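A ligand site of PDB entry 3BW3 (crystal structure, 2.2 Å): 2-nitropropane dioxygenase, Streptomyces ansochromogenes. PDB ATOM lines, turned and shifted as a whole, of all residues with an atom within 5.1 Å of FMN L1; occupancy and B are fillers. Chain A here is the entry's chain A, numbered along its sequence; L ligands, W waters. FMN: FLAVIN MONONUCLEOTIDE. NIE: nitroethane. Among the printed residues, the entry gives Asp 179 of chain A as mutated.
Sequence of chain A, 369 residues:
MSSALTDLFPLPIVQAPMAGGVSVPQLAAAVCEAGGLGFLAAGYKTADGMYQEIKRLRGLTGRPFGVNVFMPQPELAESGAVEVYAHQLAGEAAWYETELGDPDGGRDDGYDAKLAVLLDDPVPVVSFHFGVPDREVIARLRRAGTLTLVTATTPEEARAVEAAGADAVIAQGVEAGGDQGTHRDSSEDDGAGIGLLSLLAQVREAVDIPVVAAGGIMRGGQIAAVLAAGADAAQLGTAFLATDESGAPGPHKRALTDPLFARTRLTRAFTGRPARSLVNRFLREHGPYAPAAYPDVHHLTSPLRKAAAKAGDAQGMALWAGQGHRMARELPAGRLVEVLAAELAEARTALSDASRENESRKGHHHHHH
N of Gly 216 sits at hydrogen-bond distance from O2P of FMN L1, at 2.7 Å. The backbone NH (N) of Thr 238 is in hydrogen-bond range of an oxygen (O3P) of FMN L1 (3.0 Å). OG1 of Thr 238 sits at hydrogen-bond distance from O3P of FMN L1. A nitrogen (N3) of FMN L1 is in hydrogen-bond range of the side-chain amide oxygen (OD1) of Asn 68, 2.9 Å away. N of Gly 237 lies within hydrogen-bond range of O1P of FMN L1 (2.9 Å). O2' of FMN L1 sits at hydrogen-bond distance from NE2 of Gln 235, at 3.0 Å. O3' of FMN L1 lies within hydrogen-bond range of NE2 of Gln 172. O5' of FMN L1 lies within hydrogen-bond range of N of Gly 177. N5 of FMN L1 sits at hydrogen-bond distance from N of Ala 19, 3.3 Å away. An oxygen (O4) of NIE L2 is in hydrogen-bond range of the indole nitrogen (NE1) of Trp 320.
The side-chain hydroxyl of Thr 238 lies within hydrogen-bond range of the backbone NH of Gly 322 (2.9 Å). The side-chain amide nitrogen (NE2) of Gln 172 is in hydrogen-bond range of the backbone carbonyl oxygen (O) of Asp 179. N of Ala 16 sits at hydrogen-bond distance from O of Leu 236 (2.8 Å). The backbone carbonyl oxygen (O) of Trp 320 is in hydrogen-bond range of a ring nitrogen (NE2) of His 252, 2.8 Å away. The backbone carbonyl oxygen (O) of Glu 175 is in hydrogen-bond range of the backbone NH (N) of Gln 323 (3.0 Å).
The backbone carbonyl oxygen of Pro 17 lies close to a nitrogen (N5) of FMN L1, 3.4 Å away. Merely in contact with FMN L1: Ala 16 (3.5 Å), Met 18 (3.3 Å), Phe 70 (3.2 Å), His 129 (3.0 Å), Glu 175 (3.9 Å), Ala 176 (3.3 Å), Gly 178 (3.6 Å), Gly 215 (3.7 Å), Leu 236 (3.7 Å), Leu 241 (3.9 Å), Trp 320 (3.5 Å) and Gly 322 (3.4 Å). The nearest printed residue that does not touch FMN L1 is Ala 214 (4.003 Å).
Water W3 lies within hydrogen-bond range of an oxygen (O1P) of FMN L1 (2.5 Å), the backbone carbonyl oxygen (O) of Gln 235 (2.7 Å), the backbone NH (N) of Gly 215 (2.9 Å) and the backbone NH (N) of Ile 217 (3.2 Å). Water W2 lies within hydrogen-bond range of the side-chain amide oxygen (OD1) of Asn 68 (2.7 Å) and an oxygen (O4) of FMN L1 (2.8 Å). Water W1 bridges an oxygen (O3') of FMN L1 and the side-chain hydroxyl of Thr 151. Water W7 lies within hydrogen-bond range of O of Ile 217, O1P of FMN L1 and N of Gly 237. Water W6 lies within hydrogen-bond range of the side-chain hydroxyl of Thr 151 (2.6 Å), an oxygen (O2) of FMN L1 (3.4 Å) and the side-chain amide nitrogen of Asn 68 (3.5 Å). Water W4 bridges the backbone carbonyl oxygen (O) of Ala 19 (2.8 Å) and an oxygen (O4) of NIE L2 (3.5 Å).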
ATOM      1  N   ALA A  16       7.983   8.034  15.131  1.00  0.00           N
ATOM      2  CA  ALA A  16       8.840   8.457  16.231  1.00  0.00           C
ATOM      3  C   ALA A  16      10.312   8.240  15.964  1.00  0.00           C
ATOM      4  O   ALA A  16      10.707   7.245  15.338  1.00  0.00           O
ATOM      5  CB  ALA A  16       8.447   7.732  17.506  1.00  0.00           C
ATOM      6  N   PRO A  17      11.157   9.191  16.394  1.00  0.00           N
ATOM      7  CA  PRO A  17      12.593   9.004  16.169  1.00  0.00           C
ATOM      8  C   PRO A  17      12.971   7.886  17.123  1.00  0.00           C
ATOM      9  O   PRO A  17      12.527   7.876  18.271  1.00  0.00           O
ATOM     10  CB  PRO A  17      13.186  10.342  16.599  1.00  0.00           C
ATOM     11  CG  PRO A  17      12.241  10.780  17.692  1.00  0.00           C
ATOM     12  CD  PRO A  17      10.889  10.459  17.082  1.00  0.00           C
ATOM     13  N   MET A  18      13.766   6.939  16.664  1.00  0.00           N
ATOM     14  CA  MET A  18      14.179   5.838  17.515  1.00  0.00           C
ATOM     15  C   MET A  18      15.672   5.588  17.353  1.00  0.00           C
ATOM     16  O   MET A  18      16.127   5.192  16.285  1.00  0.00           O
ATOM     17  CB  MET A  18      13.365   4.588  17.166  1.00  0.00           C
ATOM     18  CG  MET A  18      11.864   4.765  17.414  1.00  0.00           C
ATOM     19  SD  MET A  18      10.866   3.346  16.957  1.00  0.00           S
ATOM     20  CE  MET A  18      10.505   3.747  15.233  1.00  0.00           C
ATOM     21  N   ALA A  19      16.419   5.845  18.420  1.00  0.00           N
ATOM     22  CA  ALA A  19      17.860   5.684  18.405  1.00  0.00           C
ATOM     23  C   ALA A  19      18.221   4.204  18.368  1.00  0.00           C
ATOM     24  O   ALA A  19      17.344   3.347  18.261  1.00  0.00           O
ATOM     25  CB  ALA A  19      18.481   6.352  19.637  1.00  0.00           C
ATOM     26  N   VAL A  22      17.678   2.310  14.692  1.00  0.00           N
ATOM     27  CA  VAL A  22      16.347   1.967  14.206  1.00  0.00           C
ATOM     28  C   VAL A  22      15.862   2.873  13.076  1.00  0.00           C
ATOM     29  O   VAL A  22      15.444   2.391  12.026  1.00  0.00           O
ATOM     30  CB  VAL A  22      15.301   2.014  15.344  1.00  0.00           C
ATOM     31  CG1 VAL A  22      13.896   1.749  14.786  1.00  0.00           C
ATOM     32  CG2 VAL A  22      15.662   0.994  16.420  1.00  0.00           C
ATOM     33  N   ALA A  41      17.004   9.973  14.163  1.00  0.00           N
ATOM     34  CA  ALA A  41      17.352  10.051  15.580  1.00  0.00           C
ATOM     35  C   ALA A  41      18.831  10.424  15.713  1.00  0.00           C
ATOM     36  O   ALA A  41      19.700   9.682  15.250  1.00  0.00           O
ATOM     37  CB  ALA A  41      17.086   8.718  16.256  1.00  0.00           C
ATOM     38  N   ASN A  68      15.585  14.356  15.776  1.00  0.00           N
ATOM     39  CA  ASN A  68      15.429  14.405  17.229  1.00  0.00           C
ATOM     40  C   ASN A  68      16.775  14.483  17.947  1.00  0.00           C
ATOM     41  O   ASN A  68      17.719  13.785  17.577  1.00  0.00           O
ATOM     42  CB  ASN A  68      14.643  13.156  17.673  1.00  0.00           C
ATOM     43  CG  ASN A  68      14.511  13.031  19.184  1.00  0.00           C
ATOM     44  OD1 ASN A  68      15.295  12.327  19.825  1.00  0.00           O
ATOM     45  ND2 ASN A  68      13.532  13.714  19.754  1.00  0.00           N
ATOM     46  N   PHE A  70      18.883  14.824  21.897  1.00  0.00           N
ATOM     47  CA  PHE A  70      18.798  14.676  23.346  1.00  0.00           C
ATOM     48  C   PHE A  70      19.348  15.914  24.042  1.00  0.00           C
ATOM     49  O   PHE A  70      20.363  16.494  23.623  1.00  0.00           O
ATOM     50  CB  PHE A  70      19.593  13.452  23.818  1.00  0.00           C
ATOM     51  CG  PHE A  70      19.048  12.133  23.343  1.00  0.00           C
ATOM     52  CD1 PHE A  70      17.767  12.025  22.803  1.00  0.00           C
ATOM     53  CD2 PHE A  70      19.810  10.976  23.477  1.00  0.00           C
ATOM     54  CE1 PHE A  70      17.251  10.785  22.418  1.00  0.00           C
ATOM     55  CE2 PHE A  70      19.307   9.739  23.096  1.00  0.00           C
ATOM     56  CZ  PHE A  70      18.023   9.638  22.562  1.00  0.00           C
ATOM     57  N   HIS A 129      14.327  15.704  23.397  1.00  0.00           N
ATOM     58  CA  HIS A 129      13.940  14.712  24.394  1.00  0.00           C
ATOM     59  C   HIS A 129      14.765  14.904  25.656  1.00  0.00           C
ATOM     60  O   HIS A 129      15.893  15.389  25.607  1.00  0.00           O
ATOM     61  CB  HIS A 129      14.163  13.294  23.844  1.00  0.00           C
ATOM     62  CG  HIS A 129      13.122  12.301  24.278  1.00  0.00           C
ATOM     63  ND1 HIS A 129      13.443  11.089  24.873  1.00  0.00           N
ATOM     64  CD2 HIS A 129      11.775  12.332  24.189  1.00  0.00           C
ATOM     65  CE1 HIS A 129      12.328  10.419  25.120  1.00  0.00           C
ATOM     66  NE2 HIS A 129      11.307  11.148  24.711  1.00  0.00           N
ATOM     67  N   THR A 151       8.997  16.841  23.982  1.00  0.00           N
ATOM     68  CA  THR A 151       8.199  15.874  24.716  1.00  0.00           C
ATOM     69  C   THR A 151       7.936  16.300  26.167  1.00  0.00           C
ATOM     70  O   THR A 151       8.836  16.793  26.852  1.00  0.00           O
ATOM     71  CB  THR A 151       8.861  14.482  24.739  1.00  0.00           C
ATOM     72  OG1 THR A 151       8.798  13.906  23.426  1.00  0.00           O
ATOM     73  CG2 THR A 151       8.169  13.563  25.732  1.00  0.00           C
ATOM     74  N   GLN A 172       3.653  12.344  25.765  1.00  0.00           N
ATOM     75  CA  GLN A 172       4.007  10.927  25.801  1.00  0.00           C
ATOM     76  C   GLN A 172       3.472  10.263  27.067  1.00  0.00           C
ATOM     77  O   GLN A 172       3.908  10.595  28.177  1.00  0.00           O
ATOM     78  CB  GLN A 172       5.526  10.772  25.724  1.00  0.00           C
ATOM     79  CG  GLN A 172       6.030   9.345  25.795  1.00  0.00           C
ATOM     80  CD  GLN A 172       7.511   9.296  26.106  1.00  0.00           C
ATOM     81  OE1 GLN A 172       7.985   9.976  27.015  1.00  0.00           O
ATOM     82  NE2 GLN A 172       8.264   8.475  25.366  1.00  0.00           N
ATOM     83  N   GLU A 175       2.297   4.369  28.392  1.00  0.00           N
ATOM     84  CA  GLU A 175       2.241   3.209  27.512  1.00  0.00           C
ATOM     85  C   GLU A 175       3.351   3.207  26.476  1.00  0.00           C
ATOM     86  O   GLU A 175       3.661   2.159  25.898  1.00  0.00           O
ATOM     87  CB  GLU A 175       0.900   3.163  26.775  1.00  0.00           C
ATOM     88  CG  GLU A 175      -0.318   3.228  27.668  1.00  0.00           C
ATOM     89  CD  GLU A 175      -0.918   4.609  27.697  1.00  0.00           C
ATOM     90  OE1 GLU A 175      -0.204   5.563  28.060  1.00  0.00           O
ATOM     91  OE2 GLU A 175      -2.108   4.739  27.344  1.00  0.00           O
ATOM     92  N   ALA A 176       3.948   4.367  26.246  1.00  0.00           N
ATOM     93  CA  ALA A 176       5.002   4.534  25.257  1.00  0.00           C
ATOM     94  C   ALA A 176       6.178   3.559  25.383  1.00  0.00           C
ATOM     95  O   ALA A 176       6.571   3.176  26.479  1.00  0.00           O
ATOM     96  CB  ALA A 176       5.528   5.976  25.283  1.00  0.00           C
ATOM     97  N   GLY A 177       6.733   3.168  24.236  1.00  0.00           N
ATOM     98  CA  GLY A 177       7.881   2.285  24.233  1.00  0.00           C
ATOM     99  C   GLY A 177       9.141   3.136  24.308  1.00  0.00           C
ATOM    100  O   GLY A 177       9.102   4.322  24.000  1.00  0.00           O
ATOM    101  N   GLY A 178      10.244   2.542  24.719  1.00  0.00           N
ATOM    102  CA  GLY A 178      11.481   3.303  24.789  1.00  0.00           C
ATOM    103  C   GLY A 178      11.593   4.300  25.937  1.00  0.00           C
ATOM    104  O   GLY A 178      10.928   4.172  26.960  1.00  0.00           O
ATOM    105  N   ASP A 179      12.452   5.293  25.748  1.00  0.00           N
ATOM    106  CA  ASP A 179      12.731   6.302  26.762  1.00  0.00           C
ATOM    107  C   ASP A 179      11.596   7.256  27.110  1.00  0.00           C
ATOM    108  O   ASP A 179      11.008   7.875  26.218  1.00  0.00           O
ATOM    109  CB  ASP A 179      13.939   7.149  26.321  1.00  0.00           C
ATOM    110  CG  ASP A 179      15.074   6.305  25.788  1.00  0.00           C
ATOM    111  OD1 ASP A 179      16.075   6.138  26.513  1.00  0.00           O
ATOM    112  OD2 ASP A 179      14.955   5.791  24.655  1.00  0.00           O
ATOM    113  N   ALA A 214       1.538  10.508  21.897  1.00  0.00           N
ATOM    114  CA  ALA A 214       2.437   9.364  21.775  1.00  0.00           C
ATOM    115  C   ALA A 214       2.274   8.335  22.884  1.00  0.00           C
ATOM    116  O   ALA A 214       2.213   8.679  24.068  1.00  0.00           O
ATOM    117  CB  ALA A 214       3.896   9.838  21.721  1.00  0.00           C
ATOM    118  N   GLY A 215       2.245   7.056  22.504  1.00  0.00           N
ATOM    119  CA  GLY A 215       2.117   6.003  23.494  1.00  0.00           C
ATOM    120  C   GLY A 215       1.098   4.927  23.181  1.00  0.00           C
ATOM    121  O   GLY A 215      -0.110   5.143  23.286  1.00  0.00           O
ATOM    122  N   GLY A 216       1.588   3.751  22.784  1.00  0.00           N
ATOM    123  CA  GLY A 216       0.721   2.623  22.489  1.00  0.00           C
ATOM    124  C   GLY A 216      -0.177   2.702  21.276  1.00  0.00           C
ATOM    125  O   GLY A 216      -1.109   1.891  21.165  1.00  0.00           O
ATOM    126  N   ILE A 217       0.066   3.628  20.357  1.00  0.00           N
ATOM    127  CA  ILE A 217      -0.783   3.747  19.175  1.00  0.00           C
ATOM    128  C   ILE A 217      -0.349   2.761  18.073  1.00  0.00           C
ATOM    129  O   ILE A 217       0.729   2.910  17.492  1.00  0.00           O
ATOM    130  CB  ILE A 217      -0.760   5.193  18.638  1.00  0.00           C
ATOM    131  CG1 ILE A 217      -1.290   6.144  19.709  1.00  0.00           C
ATOM    132  CG2 ILE A 217      -1.599   5.298  17.360  1.00  0.00           C
ATOM    133  CD1 ILE A 217      -1.094   7.630  19.413  1.00  0.00           C
ATOM    134  N   GLN A 235       2.071  10.161  17.146  1.00  0.00           N
ATOM    135  CA  GLN A 235       3.454   9.759  16.916  1.00  0.00           C
ATOM    136  C   GLN A 235       3.554   8.284  17.327  1.00  0.00           C
ATOM    137  O   GLN A 235       3.199   7.905  18.455  1.00  0.00           O
ATOM    138  CB  GLN A 235       4.417  10.615  17.754  1.00  0.00           C
ATOM    139  CG  GLN A 235       5.882  10.201  17.588  1.00  0.00           C
ATOM    140  CD  GLN A 235       6.859  11.208  18.164  1.00  0.00           C
ATOM    141  OE1 GLN A 235       6.929  12.350  17.706  1.00  0.00           O
ATOM    142  NE2 GLN A 235       7.621  10.788  19.171  1.00  0.00           N
ATOM    143  N   LEU A 236       4.017   7.466  16.392  1.00  0.00           N
ATOM    144  CA  LEU A 236       4.131   6.021  16.587  1.00  0.00           C
ATOM    145  C   LEU A 236       5.566   5.550  16.490  1.00  0.00           C
ATOM    146  O   LEU A 236       6.261   5.831  15.518  1.00  0.00           O
ATOM    147  CB  LEU A 236       3.320   5.284  15.510  1.00  0.00           C
ATOM    148  CG  LEU A 236       1.796   5.406  15.455  1.00  0.00           C
ATOM    149  CD1 LEU A 236       1.382   6.850  15.249  1.00  0.00           C
ATOM    150  CD2 LEU A 236       1.307   4.532  14.302  1.00  0.00           C
ATOM    151  N   GLY A 237       5.997   4.800  17.498  1.00  0.00           N
ATOM    152  CA  GLY A 237       7.328   4.247  17.507  1.00  0.00           C
ATOM    153  C   GLY A 237       7.283   2.755  17.242  1.00  0.00           C
ATOM    154  O   GLY A 237       7.631   2.294  16.155  1.00  0.00           O
ATOM    155  N   THR A 238       6.843   1.994  18.228  1.00  0.00           N
ATOM    156  CA  THR A 238       6.761   0.539  18.131  1.00  0.00           C
ATOM    157  C   THR A 238       6.102   0.012  16.839  1.00  0.00           C
ATOM    158  O   THR A 238       6.545  -0.995  16.292  1.00  0.00           O
ATOM    159  CB  THR A 238       6.027  -0.043  19.365  1.00  0.00           C
ATOM    160  OG1 THR A 238       6.719   0.345  20.559  1.00  0.00           O
ATOM    161  CG2 THR A 238       5.987  -1.561  19.303  1.00  0.00           C
ATOM    162  N   LEU A 241       8.695   0.153  14.358  1.00  0.00           N
ATOM    163  CA  LEU A 241       9.878  -0.586  14.793  1.00  0.00           C
ATOM    164  C   LEU A 241      10.004  -1.941  14.091  1.00  0.00           C
ATOM    165  O   LEU A 241      11.111  -2.403  13.819  1.00  0.00           O
ATOM    166  CB  LEU A 241       9.826  -0.800  16.310  1.00  0.00           C
ATOM    167  CG  LEU A 241      11.022  -1.440  17.019  1.00  0.00           C
ATOM    168  CD1 LEU A 241      12.267  -0.634  16.734  1.00  0.00           C
ATOM    169  CD2 LEU A 241      10.773  -1.493  18.506  1.00  0.00           C
ATOM    170  N   HIS A 252      15.118  -8.208  18.214  1.00  0.00           N
ATOM    171  CA  HIS A 252      14.246  -7.190  18.794  1.00  0.00           C
ATOM    172  C   HIS A 252      12.890  -7.207  18.081  1.00  0.00           C
ATOM    173  O   HIS A 252      11.839  -7.205  18.729  1.00  0.00           O
ATOM    174  CB  HIS A 252      14.906  -5.817  18.680  1.00  0.00           C
ATOM    175  CG  HIS A 252      14.197  -4.729  19.440  1.00  0.00           C
ATOM    176  ND1 HIS A 252      14.766  -3.507  19.693  1.00  0.00           N
ATOM    177  CD2 HIS A 252      12.958  -4.684  19.974  1.00  0.00           C
ATOM    178  CE1 HIS A 252      13.910  -2.745  20.342  1.00  0.00           C
ATOM    179  NE2 HIS A 252      12.796  -3.432  20.527  1.00  0.00           N
ATOM    180  N   TRP A 320      13.085  -2.313  23.713  1.00  0.00           N
ATOM    181  CA  TRP A 320      12.131  -1.193  23.763  1.00  0.00           C
ATOM    182  C   TRP A 320      10.825  -1.552  23.058  1.00  0.00           C
ATOM    183  O   TRP A 320      10.831  -2.048  21.926  1.00  0.00           O
ATOM    184  CB  TRP A 320      12.736   0.038  23.079  1.00  0.00           C
ATOM    185  CG  TRP A 320      14.051   0.509  23.618  1.00  0.00           C
ATOM    186  CD1 TRP A 320      15.099   0.979  22.881  1.00  0.00           C
ATOM    187  CD2 TRP A 320      14.449   0.590  24.995  1.00  0.00           C
ATOM    188  NE1 TRP A 320      16.129   1.349  23.709  1.00  0.00           N
ATOM    189  CE2 TRP A 320      15.758   1.127  25.009  1.00  0.00           C
ATOM    190  CE3 TRP A 320      13.825   0.273  26.206  1.00  0.00           C
ATOM    191  CZ2 TRP A 320      16.462   1.341  26.203  1.00  0.00           C
ATOM    192  CZ3 TRP A 320      14.530   0.496  27.390  1.00  0.00           C
ATOM    193  CH2 TRP A 320      15.834   1.025  27.378  1.00  0.00           C
ATOM    194  N   ALA A 321       9.704  -1.273  23.714  1.00  0.00           N
ATOM    195  CA  ALA A 321       8.386  -1.575  23.152  1.00  0.00           C
ATOM    196  C   ALA A 321       7.246  -0.979  23.968  1.00  0.00           C
ATOM    197  O   ALA A 321       7.246  -1.048  25.203  1.00  0.00           O
ATOM    198  CB  ALA A 321       8.212  -3.087  23.053  1.00  0.00           C
ATOM    199  N   GLY A 322       6.265  -0.399  23.275  1.00  0.00           N
ATOM    200  CA  GLY A 322       5.116   0.177  23.941  1.00  0.00           C
ATOM    201  C   GLY A 322       4.166  -0.945  24.300  1.00  0.00           C
ATOM    202  O   GLY A 322       4.364  -2.085  23.886  1.00  0.00           O
ATOM    203  N   GLN A 323       3.106  -0.634  25.055  1.00  0.00           N
ATOM    204  CA  GLN A 323       2.163  -1.656  25.465  1.00  0.00           C
ATOM    205  C   GLN A 323       1.344  -2.273  24.322  1.00  0.00           C
ATOM    206  O   GLN A 323       0.648  -3.259  24.515  1.00  0.00           O
ATOM    207  CB  GLN A 323       1.236  -1.095  26.553  1.00  0.00           C
ATOM    208  CG  GLN A 323       1.956  -0.622  27.813  1.00  0.00           C
ATOM    209  CD  GLN A 323       1.004  -0.190  28.909  1.00  0.00           C
ATOM    210  OE1 GLN A 323       0.048   0.535  28.663  1.00  0.00           O
ATOM    211  NE2 GLN A 323       1.268  -0.626  30.143  1.00  0.00           N
HETATM  212  N1  FMN L   1      12.016   9.155  21.488  1.00  0.00           N
HETATM  213  C2  FMN L   1      12.943  10.183  21.298  1.00  0.00           C
HETATM  214  O2  FMN L   1      12.589  11.352  21.431  1.00  0.00           O
HETATM  215  N3  FMN L   1      14.251   9.899  20.947  1.00  0.00           N
HETATM  216  C4  FMN L   1      14.711   8.599  20.768  1.00  0.00           C
HETATM  217  O4  FMN L   1      15.893   8.395  20.446  1.00  0.00           O
HETATM  218  C4A FMN L   1      13.780   7.537  20.947  1.00  0.00           C
HETATM  219  N5  FMN L   1      14.160   6.210  20.753  1.00  0.00           N
HETATM  220  C5A FMN L   1      13.236   5.169  20.894  1.00  0.00           C
HETATM  221  C6  FMN L   1      13.652   3.831  20.667  1.00  0.00           C
HETATM  222  C7  FMN L   1      12.744   2.714  20.791  1.00  0.00           C
HETATM  223  C7M FMN L   1      13.038   1.573  19.794  1.00  0.00           C
HETATM  224  C8  FMN L   1      11.388   3.059  21.124  1.00  0.00           C
HETATM  225  C8M FMN L   1      10.178   2.248  20.658  1.00  0.00           C
HETATM  226  C9  FMN L   1      10.960   4.400  21.390  1.00  0.00           C
HETATM  227  C9A FMN L   1      11.890   5.459  21.265  1.00  0.00           C
HETATM  228  N10 FMN L   1      11.505   6.805  21.483  1.00  0.00           N
HETATM  229  C10 FMN L   1      12.428   7.852  21.319  1.00  0.00           C
HETATM  230  C1' FMN L   1      10.136   7.137  22.094  1.00  0.00           C
HETATM  231  C2' FMN L   1       9.183   7.574  20.951  1.00  0.00           C
HETATM  232  O2' FMN L   1       9.399   8.943  20.658  1.00  0.00           O
HETATM  233  C3' FMN L   1       7.668   7.427  21.349  1.00  0.00           C
HETATM  234  O3' FMN L   1       7.486   8.248  22.502  1.00  0.00           O
HETATM  235  C4' FMN L   1       7.220   5.992  21.684  1.00  0.00           C
HETATM  236  O4' FMN L   1       7.775   5.107  20.700  1.00  0.00           O
HETATM  237  C5' FMN L   1       5.664   5.894  21.659  1.00  0.00           C
HETATM  238  O5' FMN L   1       5.190   4.558  21.975  1.00  0.00           O
HETATM  239  P   FMN L   1       4.888   3.326  20.914  1.00  0.00           P
HETATM  240  O1P FMN L   1       4.412   4.371  19.942  1.00  0.00           O
HETATM  241  O2P FMN L   1       4.090   2.864  22.114  1.00  0.00           O
HETATM  242  O3P FMN L   1       6.387   3.089  20.943  1.00  0.00           O
HETATM  243  N3  NIE L   2      19.456   2.936  22.441  1.00  0.00           N
HETATM  244  C1  NIE L   2      21.707   3.279  21.452  1.00  0.00           C
HETATM  245  C2  NIE L   2      20.586   2.275  21.784  1.00  0.00           C
HETATM  246  O4  NIE L   2      18.393   3.034  21.848  1.00  0.00           O
HETATM  247  O5  NIE L   2      19.556   3.374  23.572  1.00  0.00           O
HETATM  248  O   HOH W   1       8.269  11.075  22.628  1.00  0.00           O
HETATM  249  O   HOH W   2      17.163  10.487  19.026  1.00  0.00           O
HETATM  250  O   HOH W   3       2.303   5.792  19.857  1.00  0.00           O
HETATM  251  O   HOH W   4      16.492   1.061  19.732  1.00  0.00           O
HETATM  252  O   HOH W   5       2.897   0.120  21.503  1.00  0.00           O
HETATM  253  O   HOH W   6      11.005  14.241  22.116  1.00  0.00           O
HETATM  254  O   HOH W   7       3.414   2.678  17.756  1.00  0.00           O
HETATM  255  O   HOH W   8       9.991  12.222  20.557  1.00  0.00           O
HETATM  256  O   HOH W   9      16.596   5.385  22.759  1.00  0.00           O
